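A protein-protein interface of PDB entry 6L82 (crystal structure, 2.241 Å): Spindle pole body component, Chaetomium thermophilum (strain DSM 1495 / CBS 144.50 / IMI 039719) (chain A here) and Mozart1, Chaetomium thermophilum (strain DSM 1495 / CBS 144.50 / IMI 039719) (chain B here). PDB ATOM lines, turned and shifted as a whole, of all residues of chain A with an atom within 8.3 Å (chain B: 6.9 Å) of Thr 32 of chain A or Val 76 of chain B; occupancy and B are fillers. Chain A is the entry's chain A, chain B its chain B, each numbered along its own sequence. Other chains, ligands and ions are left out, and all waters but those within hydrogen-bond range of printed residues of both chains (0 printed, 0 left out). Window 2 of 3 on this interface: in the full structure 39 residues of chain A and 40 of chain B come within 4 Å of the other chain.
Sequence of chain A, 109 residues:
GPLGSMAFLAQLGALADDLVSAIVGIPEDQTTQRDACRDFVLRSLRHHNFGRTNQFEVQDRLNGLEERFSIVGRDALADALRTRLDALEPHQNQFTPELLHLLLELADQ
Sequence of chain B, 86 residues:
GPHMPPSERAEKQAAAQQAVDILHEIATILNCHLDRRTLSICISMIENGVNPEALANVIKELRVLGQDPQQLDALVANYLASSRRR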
ATOM      1  N   PRO A  27       3.978   2.443  -0.593  1.00  0.00           N
ATOM      2  CA  PRO A  27       3.148   2.530  -1.801  1.00  0.00           C
ATOM      3  C   PRO A  27       2.263   3.776  -1.874  1.00  0.00           C
ATOM      4  O   PRO A  27       1.735   4.222  -0.853  1.00  0.00           O
ATOM      5  CB  PRO A  27       2.287   1.265  -1.707  1.00  0.00           C
ATOM      6  CG  PRO A  27       3.146   0.266  -0.952  1.00  0.00           C
ATOM      7  CD  PRO A  27       4.297   1.038  -0.291  1.00  0.00           C
ATOM      8  N   GLN A  30       3.161   0.536  -4.647  1.00  0.00           N
ATOM      9  CA  GLN A  30       4.316   0.728  -5.514  1.00  0.00           C
ATOM     10  C   GLN A  30       5.410  -0.284  -5.192  1.00  0.00           C
ATOM     11  O   GLN A  30       6.396   0.044  -4.533  1.00  0.00           O
ATOM     12  CB  GLN A  30       4.840   2.157  -5.383  1.00  0.00           C
ATOM     13  CG  GLN A  30       4.613   3.005  -6.626  1.00  0.00           C
ATOM     14  CD  GLN A  30       5.682   2.801  -7.692  1.00  0.00           C
ATOM     15  OE1 GLN A  30       6.340   1.760  -7.747  1.00  0.00           O
ATOM     16  NE2 GLN A  30       5.865   3.807  -8.539  1.00  0.00           N
ATOM     17  N   THR A  31       5.224  -1.522  -5.664  1.00  0.00           N
ATOM     18  CA  THR A  31       6.168  -2.593  -5.354  1.00  0.00           C
ATOM     19  C   THR A  31       7.550  -2.306  -5.919  1.00  0.00           C
ATOM     20  O   THR A  31       8.560  -2.678  -5.312  1.00  0.00           O
ATOM     21  CB  THR A  31       5.646  -3.920  -5.905  1.00  0.00           C
ATOM     22  OG1 THR A  31       4.250  -4.049  -5.611  1.00  0.00           O
ATOM     23  CG2 THR A  31       6.396  -5.102  -5.291  1.00  0.00           C
ATOM     24  N   THR A  32       7.604  -1.636  -7.073  1.00  0.00           N
ATOM     25  CA  THR A  32       8.841  -1.497  -7.834  1.00  0.00           C
ATOM     26  C   THR A  32       9.898  -0.743  -7.045  1.00  0.00           C
ATOM     27  O   THR A  32      11.030  -1.212  -6.880  1.00  0.00           O
ATOM     28  CB  THR A  32       8.548  -0.747  -9.131  1.00  0.00           C
ATOM     29  OG1 THR A  32       7.250  -1.131  -9.611  1.00  0.00           O
ATOM     30  CG2 THR A  32       9.590  -1.089 -10.163  1.00  0.00           C
ATOM     31  N   GLN A  33       9.547   0.451  -6.572  1.00  0.00           N
ATOM     32  CA  GLN A  33      10.478   1.241  -5.784  1.00  0.00           C
ATOM     33  C   GLN A  33      11.005   0.446  -4.590  1.00  0.00           C
ATOM     34  O   GLN A  33      12.203   0.504  -4.277  1.00  0.00           O
ATOM     35  CB  GLN A  33       9.782   2.531  -5.345  1.00  0.00           C
ATOM     36  CG  GLN A  33       9.172   3.309  -6.512  1.00  0.00           C
ATOM     37  CD  GLN A  33       8.315   4.482  -6.066  1.00  0.00           C
ATOM     38  OE1 GLN A  33       7.763   4.476  -4.967  1.00  0.00           O
ATOM     39  NE2 GLN A  33       8.200   5.498  -6.921  1.00  0.00           N
ATOM     40  N   ARG A  34      10.138  -0.334  -3.937  1.00  0.00           N
ATOM     41  CA  ARG A  34      10.560  -1.038  -2.725  1.00  0.00           C
ATOM     42  C   ARG A  34      11.566  -2.142  -3.035  1.00  0.00           C
ATOM     43  O   ARG A  34      12.537  -2.332  -2.296  1.00  0.00           O
ATOM     44  CB  ARG A  34       9.342  -1.601  -1.978  1.00  0.00           C
ATOM     45  CG  ARG A  34       8.177  -0.623  -1.884  1.00  0.00           C
ATOM     46  CD  ARG A  34       8.622   0.627  -1.138  1.00  0.00           C
ATOM     47  NE  ARG A  34       7.737   1.769  -1.348  1.00  0.00           N
ATOM     48  CZ  ARG A  34       8.040   3.014  -0.991  1.00  0.00           C
ATOM     49  NH1 ARG A  34       9.204   3.278  -0.418  1.00  0.00           N
ATOM     50  NH2 ARG A  34       7.192   4.001  -1.226  1.00  0.00           N
ATOM     51  N   ASP A  35      11.372  -2.878  -4.125  1.00  0.00           N
ATOM     52  CA  ASP A  35      12.354  -3.910  -4.435  1.00  0.00           C
ATOM     53  C   ASP A  35      13.688  -3.303  -4.882  1.00  0.00           C
ATOM     54  O   ASP A  35      14.743  -3.927  -4.710  1.00  0.00           O
ATOM     55  CB  ASP A  35      11.785  -4.857  -5.488  1.00  0.00           C
ATOM     56  CG  ASP A  35      12.040  -6.320  -5.155  1.00  0.00           C
ATOM     57  OD1 ASP A  35      13.071  -6.594  -4.495  1.00  0.00           O
ATOM     58  OD2 ASP A  35      11.221  -7.189  -5.548  1.00  0.00           O
ATOM     59  N   ALA A  36      13.674  -2.082  -5.426  1.00  0.00           N
ATOM     60  CA  ALA A  36      14.927  -1.490  -5.887  1.00  0.00           C
ATOM     61  C   ALA A  36      15.723  -0.917  -4.721  1.00  0.00           C
ATOM     62  O   ALA A  36      16.953  -1.057  -4.682  1.00  0.00           O
ATOM     63  CB  ALA A  36      14.653  -0.418  -6.946  1.00  0.00           C
ATOM     64  N   CYS A  37      15.031  -0.284  -3.764  1.00  0.00           N
ATOM     65  CA  CYS A  37      15.679   0.194  -2.547  1.00  0.00           C
ATOM     66  C   CYS A  37      16.271  -0.964  -1.755  1.00  0.00           C
ATOM     67  O   CYS A  37      17.370  -0.867  -1.192  1.00  0.00           O
ATOM     68  CB  CYS A  37      14.669   0.958  -1.690  1.00  0.00           C
ATOM     69  SG  CYS A  37      14.079   2.527  -2.381  1.00  0.00           S
ATOM     70  N   ARG A  38      15.558  -2.074  -1.700  1.00  0.00           N
ATOM     71  CA  ARG A  38      16.037  -3.196  -0.912  1.00  0.00           C
ATOM     72  C   ARG A  38      17.251  -3.853  -1.552  1.00  0.00           C
ATOM     73  O   ARG A  38      18.205  -4.232  -0.866  1.00  0.00           O
ATOM     74  CB  ARG A  38      14.914  -4.194  -0.745  1.00  0.00           C
ATOM     75  CG  ARG A  38      15.393  -5.502  -0.583  1.00  0.00           C
ATOM     76  CD  ARG A  38      14.545  -6.167   0.405  1.00  0.00           C
ATOM     77  NE  ARG A  38      14.919  -7.388   0.780  1.00  0.00           N
ATOM     78  CZ  ARG A  38      14.623  -8.388   0.153  1.00  0.00           C
ATOM     79  NH1 ARG A  38      13.993  -8.298  -0.893  1.00  0.00           N
ATOM     80  NH2 ARG A  38      14.975  -9.501   0.549  1.00  0.00           N
ATOM     81  N   ASP A  39      17.210  -4.043  -2.868  1.00  0.00           N
ATOM     82  CA  ASP A  39      18.387  -4.535  -3.561  1.00  0.00           C
ATOM     83  C   ASP A  39      19.567  -3.589  -3.366  1.00  0.00           C
ATOM     84  O   ASP A  39      20.702  -4.036  -3.150  1.00  0.00           O
ATOM     85  CB  ASP A  39      18.062  -4.725  -5.046  1.00  0.00           C
ATOM     86  CG  ASP A  39      19.287  -4.931  -5.886  1.00  0.00           C
ATOM     87  OD1 ASP A  39      19.788  -6.075  -5.909  1.00  0.00           O
ATOM     88  OD2 ASP A  39      19.760  -3.945  -6.504  1.00  0.00           O
ATOM     89  N   LEU B  65      16.369   9.236  -1.434  1.00  0.00           N
ATOM     90  CA  LEU B  65      15.464   8.528  -2.338  1.00  0.00           C
ATOM     91  C   LEU B  65      14.015   8.854  -2.016  1.00  0.00           C
ATOM     92  O   LEU B  65      13.214   9.111  -2.919  1.00  0.00           O
ATOM     93  CB  LEU B  65      15.711   7.014  -2.266  1.00  0.00           C
ATOM     94  CG  LEU B  65      17.054   6.579  -2.870  1.00  0.00           C
ATOM     95  CD1 LEU B  65      17.390   5.125  -2.534  1.00  0.00           C
ATOM     96  CD2 LEU B  65      17.066   6.811  -4.399  1.00  0.00           C
ATOM     97  N   GLN B  71      15.519  10.838  -8.195  1.00  0.00           N
ATOM     98  CA  GLN B  71      16.596   9.919  -7.840  1.00  0.00           C
ATOM     99  C   GLN B  71      16.084   8.519  -7.557  1.00  0.00           C
ATOM    100  O   GLN B  71      16.783   7.539  -7.842  1.00  0.00           O
ATOM    101  CB  GLN B  71      17.376  10.463  -6.652  1.00  0.00           C
ATOM    102  CG  GLN B  71      18.230  11.653  -7.076  1.00  0.00           C
ATOM    103  CD  GLN B  71      19.110  12.141  -5.969  1.00  0.00           C
ATOM    104  OE1 GLN B  71      20.019  11.440  -5.530  1.00  0.00           O
ATOM    105  NE2 GLN B  71      18.833  13.347  -5.486  1.00  0.00           N
ATOM    106  N   LEU B  72      14.870   8.396  -7.020  1.00  0.00           N
ATOM    107  CA  LEU B  72      14.299   7.068  -6.858  1.00  0.00           C
ATOM    108  C   LEU B  72      14.016   6.439  -8.215  1.00  0.00           C
ATOM    109  O   LEU B  72      14.311   5.260  -8.435  1.00  0.00           O
ATOM    110  CB  LEU B  72      13.045   7.146  -5.990  1.00  0.00           C
ATOM    111  CG  LEU B  72      12.226   5.866  -5.812  1.00  0.00           C
ATOM    112  CD1 LEU B  72      13.070   4.700  -5.286  1.00  0.00           C
ATOM    113  CD2 LEU B  72      11.098   6.157  -4.846  1.00  0.00           C
ATOM    114  N   ASP B  73      13.498   7.223  -9.161  1.00  0.00           N
ATOM    115  CA  ASP B  73      13.295   6.676 -10.500  1.00  0.00           C
ATOM    116  C   ASP B  73      14.624   6.297 -11.148  1.00  0.00           C
ATOM    117  O   ASP B  73      14.704   5.296 -11.866  1.00  0.00           O
ATOM    118  CB  ASP B  73      12.531   7.665 -11.374  1.00  0.00           C
ATOM    119  CG  ASP B  73      12.522   7.251 -12.851  1.00  0.00           C
ATOM    120  OD1 ASP B  73      13.403   7.706 -13.615  1.00  0.00           O
ATOM    121  OD2 ASP B  73      11.634   6.452 -13.228  1.00  0.00           O
ATOM    122  N   ALA B  74      15.681   7.074 -10.895  1.00  0.00           N
ATOM    123  CA  ALA B  74      17.007   6.721 -11.404  1.00  0.00           C
ATOM    124  C   ALA B  74      17.471   5.389 -10.831  1.00  0.00           C
ATOM    125  O   ALA B  74      18.043   4.561 -11.554  1.00  0.00           O
ATOM    126  CB  ALA B  74      18.023   7.838 -11.090  1.00  0.00           C
ATOM    127  N   LEU B  75      17.208   5.155  -9.541  1.00  0.00           N
ATOM    128  CA  LEU B  75      17.459   3.850  -8.933  1.00  0.00           C
ATOM    129  C   LEU B  75      16.607   2.748  -9.572  1.00  0.00           C
ATOM    130  O   LEU B  75      17.106   1.659  -9.883  1.00  0.00           O
ATOM    131  CB  LEU B  75      17.182   3.918  -7.436  1.00  0.00           C
ATOM    132  CG  LEU B  75      17.343   2.567  -6.743  1.00  0.00           C
ATOM    133  CD1 LEU B  75      18.785   2.123  -6.889  1.00  0.00           C
ATOM    134  CD2 LEU B  75      16.933   2.607  -5.259  1.00  0.00           C
ATOM    135  N   VAL B  76      15.308   2.997  -9.751  1.00  0.00           N
ATOM    136  CA  VAL B  76      14.447   1.954 -10.305  1.00  0.00           C
ATOM    137  C   VAL B  76      14.951   1.523 -11.676  1.00  0.00           C
ATOM    138  O   VAL B  76      14.976   0.326 -12.001  1.00  0.00           O
ATOM    139  CB  VAL B  76      12.976   2.424 -10.356  1.00  0.00           C
ATOM    140  CG1 VAL B  76      12.151   1.534 -11.285  1.00  0.00           C
ATOM    141  CG2 VAL B  76      12.358   2.398  -8.969  1.00  0.00           C
ATOM    142  N   ALA B  77      15.403   2.488 -12.485  1.00  0.00           N
ATOM    143  CA  ALA B  77      15.820   2.196 -13.854  1.00  0.00           C
ATOM    144  C   ALA B  77      17.124   1.408 -13.892  1.00  0.00           C
ATOM    145  O   ALA B  77      17.273   0.494 -14.709  1.00  0.00           O
ATOM    146  CB  ALA B  77      15.962   3.496 -14.643  1.00  0.00           C
ATOM    147  N   ASN B  78      18.087   1.766 -13.037  1.00  0.00           N
ATOM    148  CA  ASN B  78      19.292   0.950 -12.905  1.00  0.00           C
ATOM    149  C   ASN B  78      18.945  -0.449 -12.406  1.00  0.00           C
ATOM    150  O   ASN B  78      19.506  -1.450 -12.872  1.00  0.00           O
ATOM    151  CB  ASN B  78      20.285   1.636 -11.955  1.00  0.00           C
ATOM    152  CG  ASN B  78      21.659   0.973 -11.957  1.00  0.00           C
ATOM    153  OD1 ASN B  78      22.325   0.928 -12.985  1.00  0.00           O
ATOM    154  ND2 ASN B  78      22.107   0.516 -10.804  1.00  0.00           N
ATOM    155  N   TYR B  79      18.003  -0.543 -11.474  1.00  0.00           N
ATOM    156  CA  TYR B  79      17.653  -1.849 -10.935  1.00  0.00           C
ATOM    157  C   TYR B  79      16.973  -2.712 -11.988  1.00  0.00           C
ATOM    158  O   TYR B  79      17.192  -3.927 -12.024  1.00  0.00           O
ATOM    159  CB  TYR B  79      16.777  -1.680  -9.704  1.00  0.00           C
ATOM    160  CG  TYR B  79      16.088  -2.944  -9.273  1.00  0.00           C
ATOM    161  CD1 TYR B  79      16.774  -3.916  -8.543  1.00  0.00           C
ATOM    162  CD2 TYR B  79      14.747  -3.169  -9.588  1.00  0.00           C
ATOM    163  CE1 TYR B  79      16.145  -5.071  -8.137  1.00  0.00           C
ATOM    164  CE2 TYR B  79      14.107  -4.328  -9.186  1.00  0.00           C
ATOM    165  CZ  TYR B  79      14.814  -5.272  -8.459  1.00  0.00           C
ATOM    166  OH  TYR B  79      14.199  -6.432  -8.052  1.00  0.00           O
ATOM    167  N   LEU B  80      16.191  -2.108 -12.886  1.00  0.00           N
ATOM    168  CA  LEU B  80      15.533  -2.912 -13.910  1.00  0.00           C
ATOM    169  C   LEU B  80      16.489  -3.313 -15.027  1.00  0.00           C
ATOM    170  O   LEU B  80      16.341  -4.398 -15.594  1.00  0.00           O
ATOM    171  CB  LEU B  80      14.333  -2.160 -14.492  1.00  0.00           C
ATOM    172  CG  LEU B  80      13.107  -1.884 -13.626  1.00  0.00           C
ATOM    173  CD1 LEU B  80      12.193  -0.920 -14.355  1.00  0.00           C
ATOM    174  CD2 LEU B  80      12.350  -3.167 -13.294  1.00  0.00           C
ATOM    175  N   ALA B  81      17.463  -2.469 -15.372  1.00  0.00           N
ATOM    176  CA  ALA B  81      18.356  -2.802 -16.484  1.00  0.00           C
ATOM    177  C   ALA B  81      19.335  -3.926 -16.119  1.00  0.00           C
ATOM    178  O   ALA B  81      19.691  -4.104 -14.943  1.00  0.00           O
ATOM    179  CB  ALA B  81      19.111  -1.566 -16.939  1.00  0.00           C
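Along chain A the printed residues that touch a printed residue of chain B span positions 32 to 39. Along chain B the printed residues that touch a printed residue of chain A span positions 72 to 79. Among the printed residues, 9 pairs touch across the chains.
NE2 of Gln 30 of chain A sits close to NE2 of Gln 33 of chain A (3.3 Å). The backbone carbonyl oxygen (O) of Gln 33 of chain A is in hydrogen-bond range of the side-chain sulfur (SG) of Cys 37 of chain A (3.3 Å).
Of chain B, only Val 76 comes within 4 Å of Thr 32 of chain A. Val 76 of chain B touches just these residues of chain A: Thr 32 (3.8 Å) and Gln 33 (3.9 Å). No residue of chain A comes within 4 Å of Ala 77 of chain B. Of the printed residues of chain A, Tyr 79 of chain B touches Asp 35 (3.6 Å), Ala 36 (3.7 Å) and Asp 39 (3.6 Å). Of the printed residues of chain A, Leu 75 of chain B touches Ala 36 and Cys 37. Of the printed residues of chain B, Asp 39 of chain A touches Tyr 79. Printed residues of chain B within 4 Å of Ala 36 of chain A: Leu 75 and Tyr 79. Leu 65 of chain B touches none of the printed residues of chain A. The nearest residue of chain B that does not touch Thr 32 of chain A is Leu 80 of chain B (4.7 Å). The nearest residue of chain A that does not touch Val 76 of chain B is Ala 36 of chain A (4.1 Å).
Among the printed residues, pairs that only touch across the chains: Thr 32 of chain A with Val 76 of chain B (3.8 Å), Gln 33 of chain A with Leu 72 of chain B (3.5 Å), Gln 33 of chain A with Val 76 of chain B (3.9 Å), Asp 35 of chain A with Tyr 79 of chain B (3.6 Å), Ala 36 of chain A with Leu 75 of chain B (3.7 Å), Ala 36 of chain A with Tyr 79 of chain B (3.7 Å), Cys 37 of chain A with Leu 72 of chain B (3.8 Å), Cys 37 of chain A with Leu 75 of chain B (3.8 Å) and Asp 39 of chain A with Tyr 79 of chain B (3.6 Å).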
